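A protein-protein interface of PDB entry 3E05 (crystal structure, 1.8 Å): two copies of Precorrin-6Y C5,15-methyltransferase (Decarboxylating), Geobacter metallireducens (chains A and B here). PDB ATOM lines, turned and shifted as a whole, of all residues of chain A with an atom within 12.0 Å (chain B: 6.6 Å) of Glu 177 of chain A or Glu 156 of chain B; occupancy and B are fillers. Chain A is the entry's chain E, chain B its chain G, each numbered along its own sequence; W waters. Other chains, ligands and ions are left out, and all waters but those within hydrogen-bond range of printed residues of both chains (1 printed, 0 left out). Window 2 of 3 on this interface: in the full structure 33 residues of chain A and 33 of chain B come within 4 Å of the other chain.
The backbone carbonyl oxygen (O) of Lys 173 of chain A lies close to the backbone carbonyl oxygen (O) of Val 162 of chain B, at 3.3 Å. OE2 of Glu 156 of chain B lies close to O of Leu 175 of chain A. OE1 of Glu 177 of chain A sits close to OE1 of Glu 156 of chain B (3.3 Å). OG1 of Thr 176 of chain A is in hydrogen-bond range of O of Val 162 of chain B (2.7 Å).
The side-chain hydroxyl (OG1) of Thr 172 of chain A sits at hydrogen-bond distance from the side-chain hydroxyl (OG1) of Thr 176 of chain A (3.4 Å).
O of Lys 173 of chain A touches CE of Met 161 of chain B, at 3.8 Å. Met 161 of chain B touches Gly 174 of chain A. Thr 176 of chain A touches Val 152 of chain B. Thr 176 of chain A touches Glu 156 of chain B. Val 152 of chain B touches Glu 177 of chain A (CG1 to CD, 3.9 Å).
Ala 170 of chain A touches none of the printed residues of chain B. Of the printed residues of chain B, Lys 173 of chain A touches Met 161 (3.8 Å) and Val 162 (3.3 Å). Of the printed residues of chain B, Gly 174 of chain A touches Met 161. Of the printed residues of chain B, Thr 176 of chain A touches Val 152 (3.6 Å), Glu 156 (3.3 Å) and Val 162 (2.7 Å). Of chain B, only Val 152 (3.9 Å) and Glu 156 (3.3 Å) come within 4 Å of Glu 177 of chain A. Met 180 of chain A touches none of the printed residues of chain B. No residue of chain A comes within 4 Å of Thr 149 of chain B. Printed residues of chain A within 4 Å of Val 152 of chain B: Thr 176 (3.6 Å) and Glu 177 (3.9 Å). No residue of chain A comes within 4 Å of Leu 155 of chain B. Of chain A, only Leu 175 (3.0 Å), Thr 176 (3.3 Å) and Glu 177 (3.3 Å) come within 4 Å of Glu 156 of chain B. Asp 157 of chain B touches none of the printed residues of chain A. No residue of chain A comes within 4 Å of His 158 of chain B. No residue of chain A comes within 4 Å of Gly 159 of chain B. Val 162 of chain B touches two residues of chain A. The nearest residue of chain B that does not touch Glu 177 of chain A is Glu 153 of chain B (4.1 Å). The nearest printed residue of chain B that does not touch Thr 176 of chain A is Met 161 of chain B (5.1 Å).
Hydrophobic or aromatic side chains of chain B that line the printed part of chain A: Val 152, Met 161 and Val 162. Along chain B the printed residues that touch a printed residue of chain A span positions 152 to 162. Among the printed residues, no Asp or Glu carboxylate lies within 4 Å of a Lys or Arg side-chain nitrogen of the other chain.
No position is printed for both chains. Of the 9 pairs that touch across the chains among the printed residues, none has its exchanged pair printed and touching as well.
Water W1 lies within hydrogen-bond range of the backbone carbonyl oxygen (O) of Gly 174 of chain A, the side-chain carboxylate (OE2) of Glu 156 of chain B and the backbone NH (N) of Val 162 of chain B.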
ATOM      1  N   ALA A 170       0.651 -10.743 -17.173  1.00  0.00           N
ATOM      2  CA  ALA A 170       1.863 -10.241 -16.505  1.00  0.00           C
ATOM      3  C   ALA A 170       2.671 -11.435 -15.981  1.00  0.00           C
ATOM      4  O   ALA A 170       2.114 -12.282 -15.301  1.00  0.00           O
ATOM      5  CB  ALA A 170       1.502  -9.327 -15.385  1.00  0.00           C
ATOM      6  N   LYS A 171       3.966 -11.480 -16.303  1.00  0.00           N
ATOM      7  CA  LYS A 171       4.835 -12.627 -16.004  1.00  0.00           C
ATOM      8  C   LYS A 171       6.071 -12.302 -15.174  1.00  0.00           C
ATOM      9  O   LYS A 171       6.653 -11.234 -15.302  1.00  0.00           O
ATOM     10  CB  LYS A 171       5.329 -13.305 -17.283  1.00  0.00           C
ATOM     11  CG  LYS A 171       4.278 -13.614 -18.327  1.00  0.00           C
ATOM     12  CD  LYS A 171       4.649 -14.880 -19.094  1.00  0.00           C
ATOM     13  CE  LYS A 171       5.909 -14.740 -19.913  1.00  0.00           C
ATOM     14  NZ  LYS A 171       5.862 -15.668 -21.057  1.00  0.00           N
ATOM     15  N   THR A 172       6.459 -13.251 -14.331  1.00  0.00           N
ATOM     16  CA  THR A 172       7.771 -13.280 -13.731  1.00  0.00           C
ATOM     17  C   THR A 172       8.651 -14.160 -14.619  1.00  0.00           C
ATOM     18  O   THR A 172       8.201 -15.184 -15.139  1.00  0.00           O
ATOM     19  CB  THR A 172       7.745 -13.966 -12.370  1.00  0.00           C
ATOM     20  OG1 THR A 172       7.506 -15.369 -12.573  1.00  0.00           O
ATOM     21  CG2 THR A 172       6.673 -13.382 -11.468  1.00  0.00           C
ATOM     22  N   LYS A 173       9.848 -13.655 -14.863  1.00  0.00           N
ATOM     23  CA  LYS A 173      10.942 -14.385 -15.486  1.00  0.00           C
ATOM     24  C   LYS A 173      11.320 -15.518 -14.568  1.00  0.00           C
ATOM     25  O   LYS A 173      10.790 -16.588 -14.728  1.00  0.00           O
ATOM     26  CB  LYS A 173      12.145 -13.471 -15.736  1.00  0.00           C
ATOM     27  CG  LYS A 173      12.849 -13.678 -17.076  1.00  0.00           C
ATOM     28  CD  LYS A 173      14.365 -13.769 -16.939  1.00  0.00           C
ATOM     29  CE  LYS A 173      15.099 -13.158 -18.125  1.00  0.00           C
ATOM     30  NZ  LYS A 173      15.627 -11.830 -17.809  1.00  0.00           N
ATOM     31  N   GLY A 174      12.185 -15.251 -13.589  1.00  0.00           N
ATOM     32  CA  GLY A 174      13.217 -16.186 -13.183  1.00  0.00           C
ATOM     33  C   GLY A 174      13.700 -16.298 -11.736  1.00  0.00           C
ATOM     34  O   GLY A 174      13.719 -17.378 -11.198  1.00  0.00           O
ATOM     35  N   LEU A 175      14.077 -15.210 -11.082  1.00  0.00           N
ATOM     36  CA  LEU A 175      14.146 -15.317  -9.634  1.00  0.00           C
ATOM     37  C   LEU A 175      12.789 -15.573  -8.985  1.00  0.00           C
ATOM     38  O   LEU A 175      12.694 -16.214  -7.956  1.00  0.00           O
ATOM     39  CB  LEU A 175      14.997 -14.244  -8.953  1.00  0.00           C
ATOM     40  CG  LEU A 175      16.222 -14.982  -8.382  1.00  0.00           C
ATOM     41  CD1 LEU A 175      17.469 -14.141  -8.093  1.00  0.00           C
ATOM     42  CD2 LEU A 175      15.859 -15.867  -7.203  1.00  0.00           C
ATOM     43  N   THR A 176      11.741 -15.152  -9.663  1.00  0.00           N
ATOM     44  CA  THR A 176      10.377 -15.327  -9.197  1.00  0.00           C
ATOM     45  C   THR A 176       9.823 -14.471  -8.087  1.00  0.00           C
ATOM     46  O   THR A 176       9.034 -13.597  -8.354  1.00  0.00           O
ATOM     47  CB  THR A 176       9.803 -16.734  -9.300  1.00  0.00           C
ATOM     48  OG1 THR A 176       9.746 -17.120 -10.660  1.00  0.00           O
ATOM     49  CG2 THR A 176       8.441 -16.749  -8.838  1.00  0.00           C
ATOM     50  N   GLU A 177      10.235 -14.692  -6.848  1.00  0.00           N
ATOM     51  CA  GLU A 177       9.775 -13.811  -5.790  1.00  0.00           C
ATOM     52  C   GLU A 177      10.466 -12.445  -5.685  1.00  0.00           C
ATOM     53  O   GLU A 177       9.914 -11.508  -5.167  1.00  0.00           O
ATOM     54  CB  GLU A 177       9.681 -14.477  -4.427  1.00  0.00           C
ATOM     55  CG  GLU A 177      10.333 -15.754  -4.250  1.00  0.00           C
ATOM     56  CD  GLU A 177       9.580 -16.555  -3.227  1.00  0.00           C
ATOM     57  OE1 GLU A 177      10.048 -17.638  -2.798  1.00  0.00           O
ATOM     58  OE2 GLU A 177       8.489 -16.066  -2.846  1.00  0.00           O
ATOM     59  N   TYR A 178      11.702 -12.374  -6.143  1.00  0.00           N
ATOM     60  CA  TYR A 178      12.522 -11.159  -6.011  1.00  0.00           C
ATOM     61  C   TYR A 178      12.464 -10.374  -7.313  1.00  0.00           C
ATOM     62  O   TYR A 178      13.390  -9.653  -7.696  1.00  0.00           O
ATOM     63  CB  TYR A 178      13.952 -11.546  -5.643  1.00  0.00           C
ATOM     64  CG  TYR A 178      14.000 -12.474  -4.450  1.00  0.00           C
ATOM     65  CD1 TYR A 178      13.826 -11.982  -3.154  1.00  0.00           C
ATOM     66  CD2 TYR A 178      14.193 -13.848  -4.618  1.00  0.00           C
ATOM     67  CE1 TYR A 178      13.859 -12.832  -2.052  1.00  0.00           C
ATOM     68  CE2 TYR A 178      14.222 -14.706  -3.525  1.00  0.00           C
ATOM     69  CZ  TYR A 178      14.057 -14.194  -2.245  1.00  0.00           C
ATOM     70  OH  TYR A 178      14.088 -15.045  -1.160  1.00  0.00           O
ATOM     71  N   LYS A 179      11.333 -10.513  -8.000  1.00  0.00           N
ATOM     72  CA  LYS A 179      11.263 -10.273  -9.436  1.00  0.00           C
ATOM     73  C   LYS A 179       9.902  -9.709  -9.833  1.00  0.00           C
ATOM     74  O   LYS A 179       8.875 -10.373  -9.685  1.00  0.00           O
ATOM     75  CB  LYS A 179      11.545 -11.563 -10.209  1.00  0.00           C
ATOM     76  CG  LYS A 179      12.979 -11.694 -10.697  1.00  0.00           C
ATOM     77  CD  LYS A 179      13.097 -11.328 -12.167  1.00  0.00           C
ATOM     78  CE  LYS A 179      11.854 -11.738 -12.940  1.00  0.00           C
ATOM     79  NZ  LYS A 179      11.170 -10.566 -13.553  1.00  0.00           N
ATOM     80  N   MET A 180       9.905  -8.481 -10.340  1.00  0.00           N
ATOM     81  CA  MET A 180       8.678  -7.779 -10.684  1.00  0.00           C
ATOM     82  C   MET A 180       7.908  -8.510 -11.787  1.00  0.00           C
ATOM     83  O   MET A 180       8.507  -9.144 -12.658  1.00  0.00           O
ATOM     84  CB  MET A 180       8.953  -6.310 -11.036  1.00  0.00           C
ATOM     85  CG  MET A 180       9.506  -6.033 -12.421  1.00  0.00           C
ATOM     86  SD  MET A 180      10.161  -4.362 -12.601  1.00  0.00           S
ATOM     87  CE  MET A 180       8.749  -3.345 -12.214  1.00  0.00           C
ATOM     88  N   PHE A 181       6.581  -8.446 -11.724  1.00  0.00           N
ATOM     89  CA  PHE A 181       5.755  -8.900 -12.843  1.00  0.00           C
ATOM     90  C   PHE A 181       5.907  -7.895 -13.964  1.00  0.00           C
ATOM     91  O   PHE A 181       5.781  -6.677 -13.746  1.00  0.00           O
ATOM     92  CB  PHE A 181       4.282  -8.966 -12.456  1.00  0.00           C
ATOM     93  CG  PHE A 181       3.919 -10.161 -11.653  1.00  0.00           C
ATOM     94  CD1 PHE A 181       3.416 -11.301 -12.274  1.00  0.00           C
ATOM     95  CD2 PHE A 181       4.081 -10.148 -10.264  1.00  0.00           C
ATOM     96  CE1 PHE A 181       3.064 -12.421 -11.510  1.00  0.00           C
ATOM     97  CE2 PHE A 181       3.747 -11.261  -9.495  1.00  0.00           C
ATOM     98  CZ  PHE A 181       3.238 -12.397 -10.116  1.00  0.00           C
ATOM     99  N   GLU A 182       6.192  -8.401 -15.153  1.00  0.00           N
ATOM    100  CA  GLU A 182       6.247  -7.553 -16.331  1.00  0.00           C
ATOM    101  C   GLU A 182       5.039  -7.810 -17.210  1.00  0.00           C
ATOM    102  O   GLU A 182       4.833  -8.923 -17.655  1.00  0.00           O
ATOM    103  CB  GLU A 182       7.544  -7.800 -17.078  1.00  0.00           C
ATOM    104  CG  GLU A 182       8.755  -7.542 -16.194  1.00  0.00           C
ATOM    105  CD  GLU A 182       9.972  -7.142 -16.981  1.00  0.00           C
ATOM    106  OE1 GLU A 182      10.523  -6.062 -16.689  1.00  0.00           O
ATOM    107  OE2 GLU A 182      10.369  -7.900 -17.891  1.00  0.00           O
ATOM    108  N   THR B 149       1.846 -17.894  -2.989  1.00  0.00           N
ATOM    109  CA  THR B 149       2.998 -17.770  -2.089  1.00  0.00           C
ATOM    110  C   THR B 149       3.659 -19.120  -1.867  1.00  0.00           C
ATOM    111  O   THR B 149       4.858 -19.286  -2.113  1.00  0.00           O
ATOM    112  CB  THR B 149       2.538 -17.231  -0.686  1.00  0.00           C
ATOM    113  OG1 THR B 149       2.090 -15.879  -0.809  1.00  0.00           O
ATOM    114  CG2 THR B 149       3.644 -17.298   0.348  1.00  0.00           C
ATOM    115  N   ALA B 151       3.047 -22.223  -3.275  1.00  0.00           N
ATOM    116  CA  ALA B 151       3.430 -22.995  -4.446  1.00  0.00           C
ATOM    117  C   ALA B 151       4.813 -22.578  -4.923  1.00  0.00           C
ATOM    118  O   ALA B 151       5.690 -23.432  -5.084  1.00  0.00           O
ATOM    119  CB  ALA B 151       2.407 -22.848  -5.560  1.00  0.00           C
ATOM    120  N   VAL B 152       5.007 -21.269  -5.095  1.00  0.00           N
ATOM    121  CA  VAL B 152       6.288 -20.710  -5.533  1.00  0.00           C
ATOM    122  C   VAL B 152       7.438 -21.095  -4.593  1.00  0.00           C
ATOM    123  O   VAL B 152       8.466 -21.615  -5.045  1.00  0.00           O
ATOM    124  CB  VAL B 152       6.194 -19.173  -5.712  1.00  0.00           C
ATOM    125  CG1 VAL B 152       7.574 -18.552  -5.844  1.00  0.00           C
ATOM    126  CG2 VAL B 152       5.318 -18.846  -6.921  1.00  0.00           C
ATOM    127  N   GLU B 153       7.224 -20.883  -3.294  1.00  0.00           N
ATOM    128  CA  GLU B 153       8.181 -21.255  -2.262  1.00  0.00           C
ATOM    129  C   GLU B 153       8.558 -22.740  -2.378  1.00  0.00           C
ATOM    130  O   GLU B 153       9.732 -23.052  -2.577  1.00  0.00           O
ATOM    131  CB  GLU B 153       7.614 -20.937  -0.871  1.00  0.00           C
ATOM    132  CG  GLU B 153       8.583 -21.211   0.279  1.00  0.00           C
ATOM    133  CD  GLU B 153       7.941 -21.079   1.655  1.00  0.00           C
ATOM    134  OE1 GLU B 153       6.825 -20.521   1.755  1.00  0.00           O
ATOM    135  OE2 GLU B 153       8.563 -21.537   2.642  1.00  0.00           O
ATOM    136  N   PHE B 154       7.558 -23.625  -2.320  1.00  0.00           N
ATOM    137  CA  PHE B 154       7.784 -25.076  -2.326  1.00  0.00           C
ATOM    138  C   PHE B 154       8.399 -25.580  -3.630  1.00  0.00           C
ATOM    139  O   PHE B 154       9.230 -26.478  -3.613  1.00  0.00           O
ATOM    140  CB  PHE B 154       6.499 -25.866  -2.027  1.00  0.00           C
ATOM    141  CG  PHE B 154       5.823 -25.500  -0.729  1.00  0.00           C
ATOM    142  CD1 PHE B 154       6.558 -25.127   0.395  1.00  0.00           C
ATOM    143  CD2 PHE B 154       4.441 -25.564  -0.625  1.00  0.00           C
ATOM    144  CE1 PHE B 154       5.924 -24.792   1.581  1.00  0.00           C
ATOM    145  CE2 PHE B 154       3.796 -25.226   0.559  1.00  0.00           C
ATOM    146  CZ  PHE B 154       4.540 -24.845   1.670  1.00  0.00           C
ATOM    147  N   LEU B 155       8.004 -25.000  -4.760  1.00  0.00           N
ATOM    148  CA  LEU B 155       8.601 -25.401  -6.030  1.00  0.00           C
ATOM    149  C   LEU B 155      10.062 -25.002  -6.153  1.00  0.00           C
ATOM    150  O   LEU B 155      10.881 -25.777  -6.651  1.00  0.00           O
ATOM    151  CB  LEU B 155       7.799 -24.875  -7.215  1.00  0.00           C
ATOM    152  CG  LEU B 155       6.453 -25.546  -7.460  1.00  0.00           C
ATOM    153  CD1 LEU B 155       5.654 -24.681  -8.413  1.00  0.00           C
ATOM    154  CD2 LEU B 155       6.611 -26.969  -7.987  1.00  0.00           C
ATOM    155  N   GLU B 156      10.396 -23.809  -5.675  1.00  0.00           N
ATOM    156  CA  GLU B 156      11.777 -23.342  -5.705  1.00  0.00           C
ATOM    157  C   GLU B 156      12.621 -24.070  -4.667  1.00  0.00           C
ATOM    158  O   GLU B 156      13.817 -24.285  -4.887  1.00  0.00           O
ATOM    159  CB  GLU B 156      11.853 -21.823  -5.528  1.00  0.00           C
ATOM    160  CG  GLU B 156      11.322 -21.094  -6.733  1.00  0.00           C
ATOM    161  CD  GLU B 156      11.458 -19.591  -6.660  1.00  0.00           C
ATOM    162  OE1 GLU B 156      11.349 -19.010  -5.560  1.00  0.00           O
ATOM    163  OE2 GLU B 156      11.661 -18.997  -7.735  1.00  0.00           O
ATOM    164  N   ASP B 157      11.984 -24.465  -3.560  1.00  0.00           N
ATOM    165  CA  ASP B 157      12.604 -25.315  -2.541  1.00  0.00           C
ATOM    166  C   ASP B 157      13.159 -26.595  -3.153  1.00  0.00           C
ATOM    167  O   ASP B 157      14.272 -26.995  -2.852  1.00  0.00           O
ATOM    168  CB  ASP B 157      11.599 -25.677  -1.441  1.00  0.00           C
ATOM    169  CG  ASP B 157      11.436 -24.581  -0.400  1.00  0.00           C
ATOM    170  OD1 ASP B 157      12.158 -23.559  -0.480  1.00  0.00           O
ATOM    171  OD2 ASP B 157      10.577 -24.753   0.496  1.00  0.00           O
ATOM    172  N   HIS B 158      12.385 -27.207  -4.043  1.00  0.00           N
ATOM    173  CA  HIS B 158      12.767 -28.449  -4.701  1.00  0.00           C
ATOM    174  C   HIS B 158      13.646 -28.271  -5.949  1.00  0.00           C
ATOM    175  O   HIS B 158      13.916 -29.238  -6.659  1.00  0.00           O
ATOM    176  CB  HIS B 158      11.510 -29.253  -5.032  1.00  0.00           C
ATOM    177  CG  HIS B 158      10.805 -29.787  -3.823  1.00  0.00           C
ATOM    178  ND1 HIS B 158       9.630 -29.249  -3.346  1.00  0.00           N
ATOM    179  CD2 HIS B 158      11.113 -30.812  -2.993  1.00  0.00           C
ATOM    180  CE1 HIS B 158       9.245 -29.917  -2.272  1.00  0.00           C
ATOM    181  NE2 HIS B 158      10.127 -30.873  -2.039  1.00  0.00           N
ATOM    182  N   GLY B 159      14.071 -27.038  -6.219  1.00  0.00           N
ATOM    183  CA  GLY B 159      15.014 -26.746  -7.302  1.00  0.00           C
ATOM    184  C   GLY B 159      14.401 -26.564  -8.681  1.00  0.00           C
ATOM    185  O   GLY B 159      15.057 -26.815  -9.696  1.00  0.00           O
ATOM    186  N   TYR B 160      13.140 -26.135  -8.727  1.00  0.00           N
ATOM    187  CA  TYR B 160      12.469 -25.881  -9.997  1.00  0.00           C
ATOM    188  C   TYR B 160      12.652 -24.427 -10.389  1.00  0.00           C
ATOM    189  O   TYR B 160      12.661 -23.538  -9.527  1.00  0.00           O
ATOM    190  CB  TYR B 160      10.959 -26.185  -9.917  1.00  0.00           C
ATOM    191  CG  TYR B 160      10.621 -27.659  -9.831  1.00  0.00           C
ATOM    192  CD1 TYR B 160      10.301 -28.382 -10.971  1.00  0.00           C
ATOM    193  CD2 TYR B 160      10.625 -28.325  -8.605  1.00  0.00           C
ATOM    194  CE1 TYR B 160      10.003 -29.739 -10.897  1.00  0.00           C
ATOM    195  CE2 TYR B 160      10.335 -29.681  -8.519  1.00  0.00           C
ATOM    196  CZ  TYR B 160      10.030 -30.383  -9.666  1.00  0.00           C
ATOM    197  OH  TYR B 160       9.723 -31.726  -9.594  1.00  0.00           O
ATOM    198  N   MET B 161      12.832 -24.209 -11.688  1.00  0.00           N
ATOM    199  CA  MET B 161      12.688 -22.878 -12.263  1.00  0.00           C
ATOM    200  C   MET B 161      11.202 -22.603 -12.424  1.00  0.00           C
ATOM    201  O   MET B 161      10.476 -23.411 -13.013  1.00  0.00           O
ATOM    202  CB  MET B 161      13.407 -22.775 -13.609  1.00  0.00           C
ATOM    203  CG  MET B 161      14.614 -21.835 -13.595  1.00  0.00           C
ATOM    204  SD  MET B 161      14.392 -20.324 -14.564  1.00  0.00           S
ATOM    205  CE  MET B 161      12.922 -19.598 -13.855  1.00  0.00           C
ATOM    206  N   VAL B 162      10.751 -21.477 -11.876  1.00  0.00           N
ATOM    207  CA  VAL B 162       9.333 -21.156 -11.805  1.00  0.00           C
ATOM    208  C   VAL B 162       8.998 -19.918 -12.639  1.00  0.00           C
ATOM    209  O   VAL B 162       9.715 -18.919 -12.610  1.00  0.00           O
ATOM    210  CB  VAL B 162       8.872 -20.999 -10.325  1.00  0.00           C
ATOM    211  CG1 VAL B 162       7.394 -20.627 -10.214  1.00  0.00           C
ATOM    212  CG2 VAL B 162       9.119 -22.298  -9.554  1.00  0.00           C
HETATM  213  O   HOH W   1      12.557 -19.554 -10.306  1.00  0.00           O
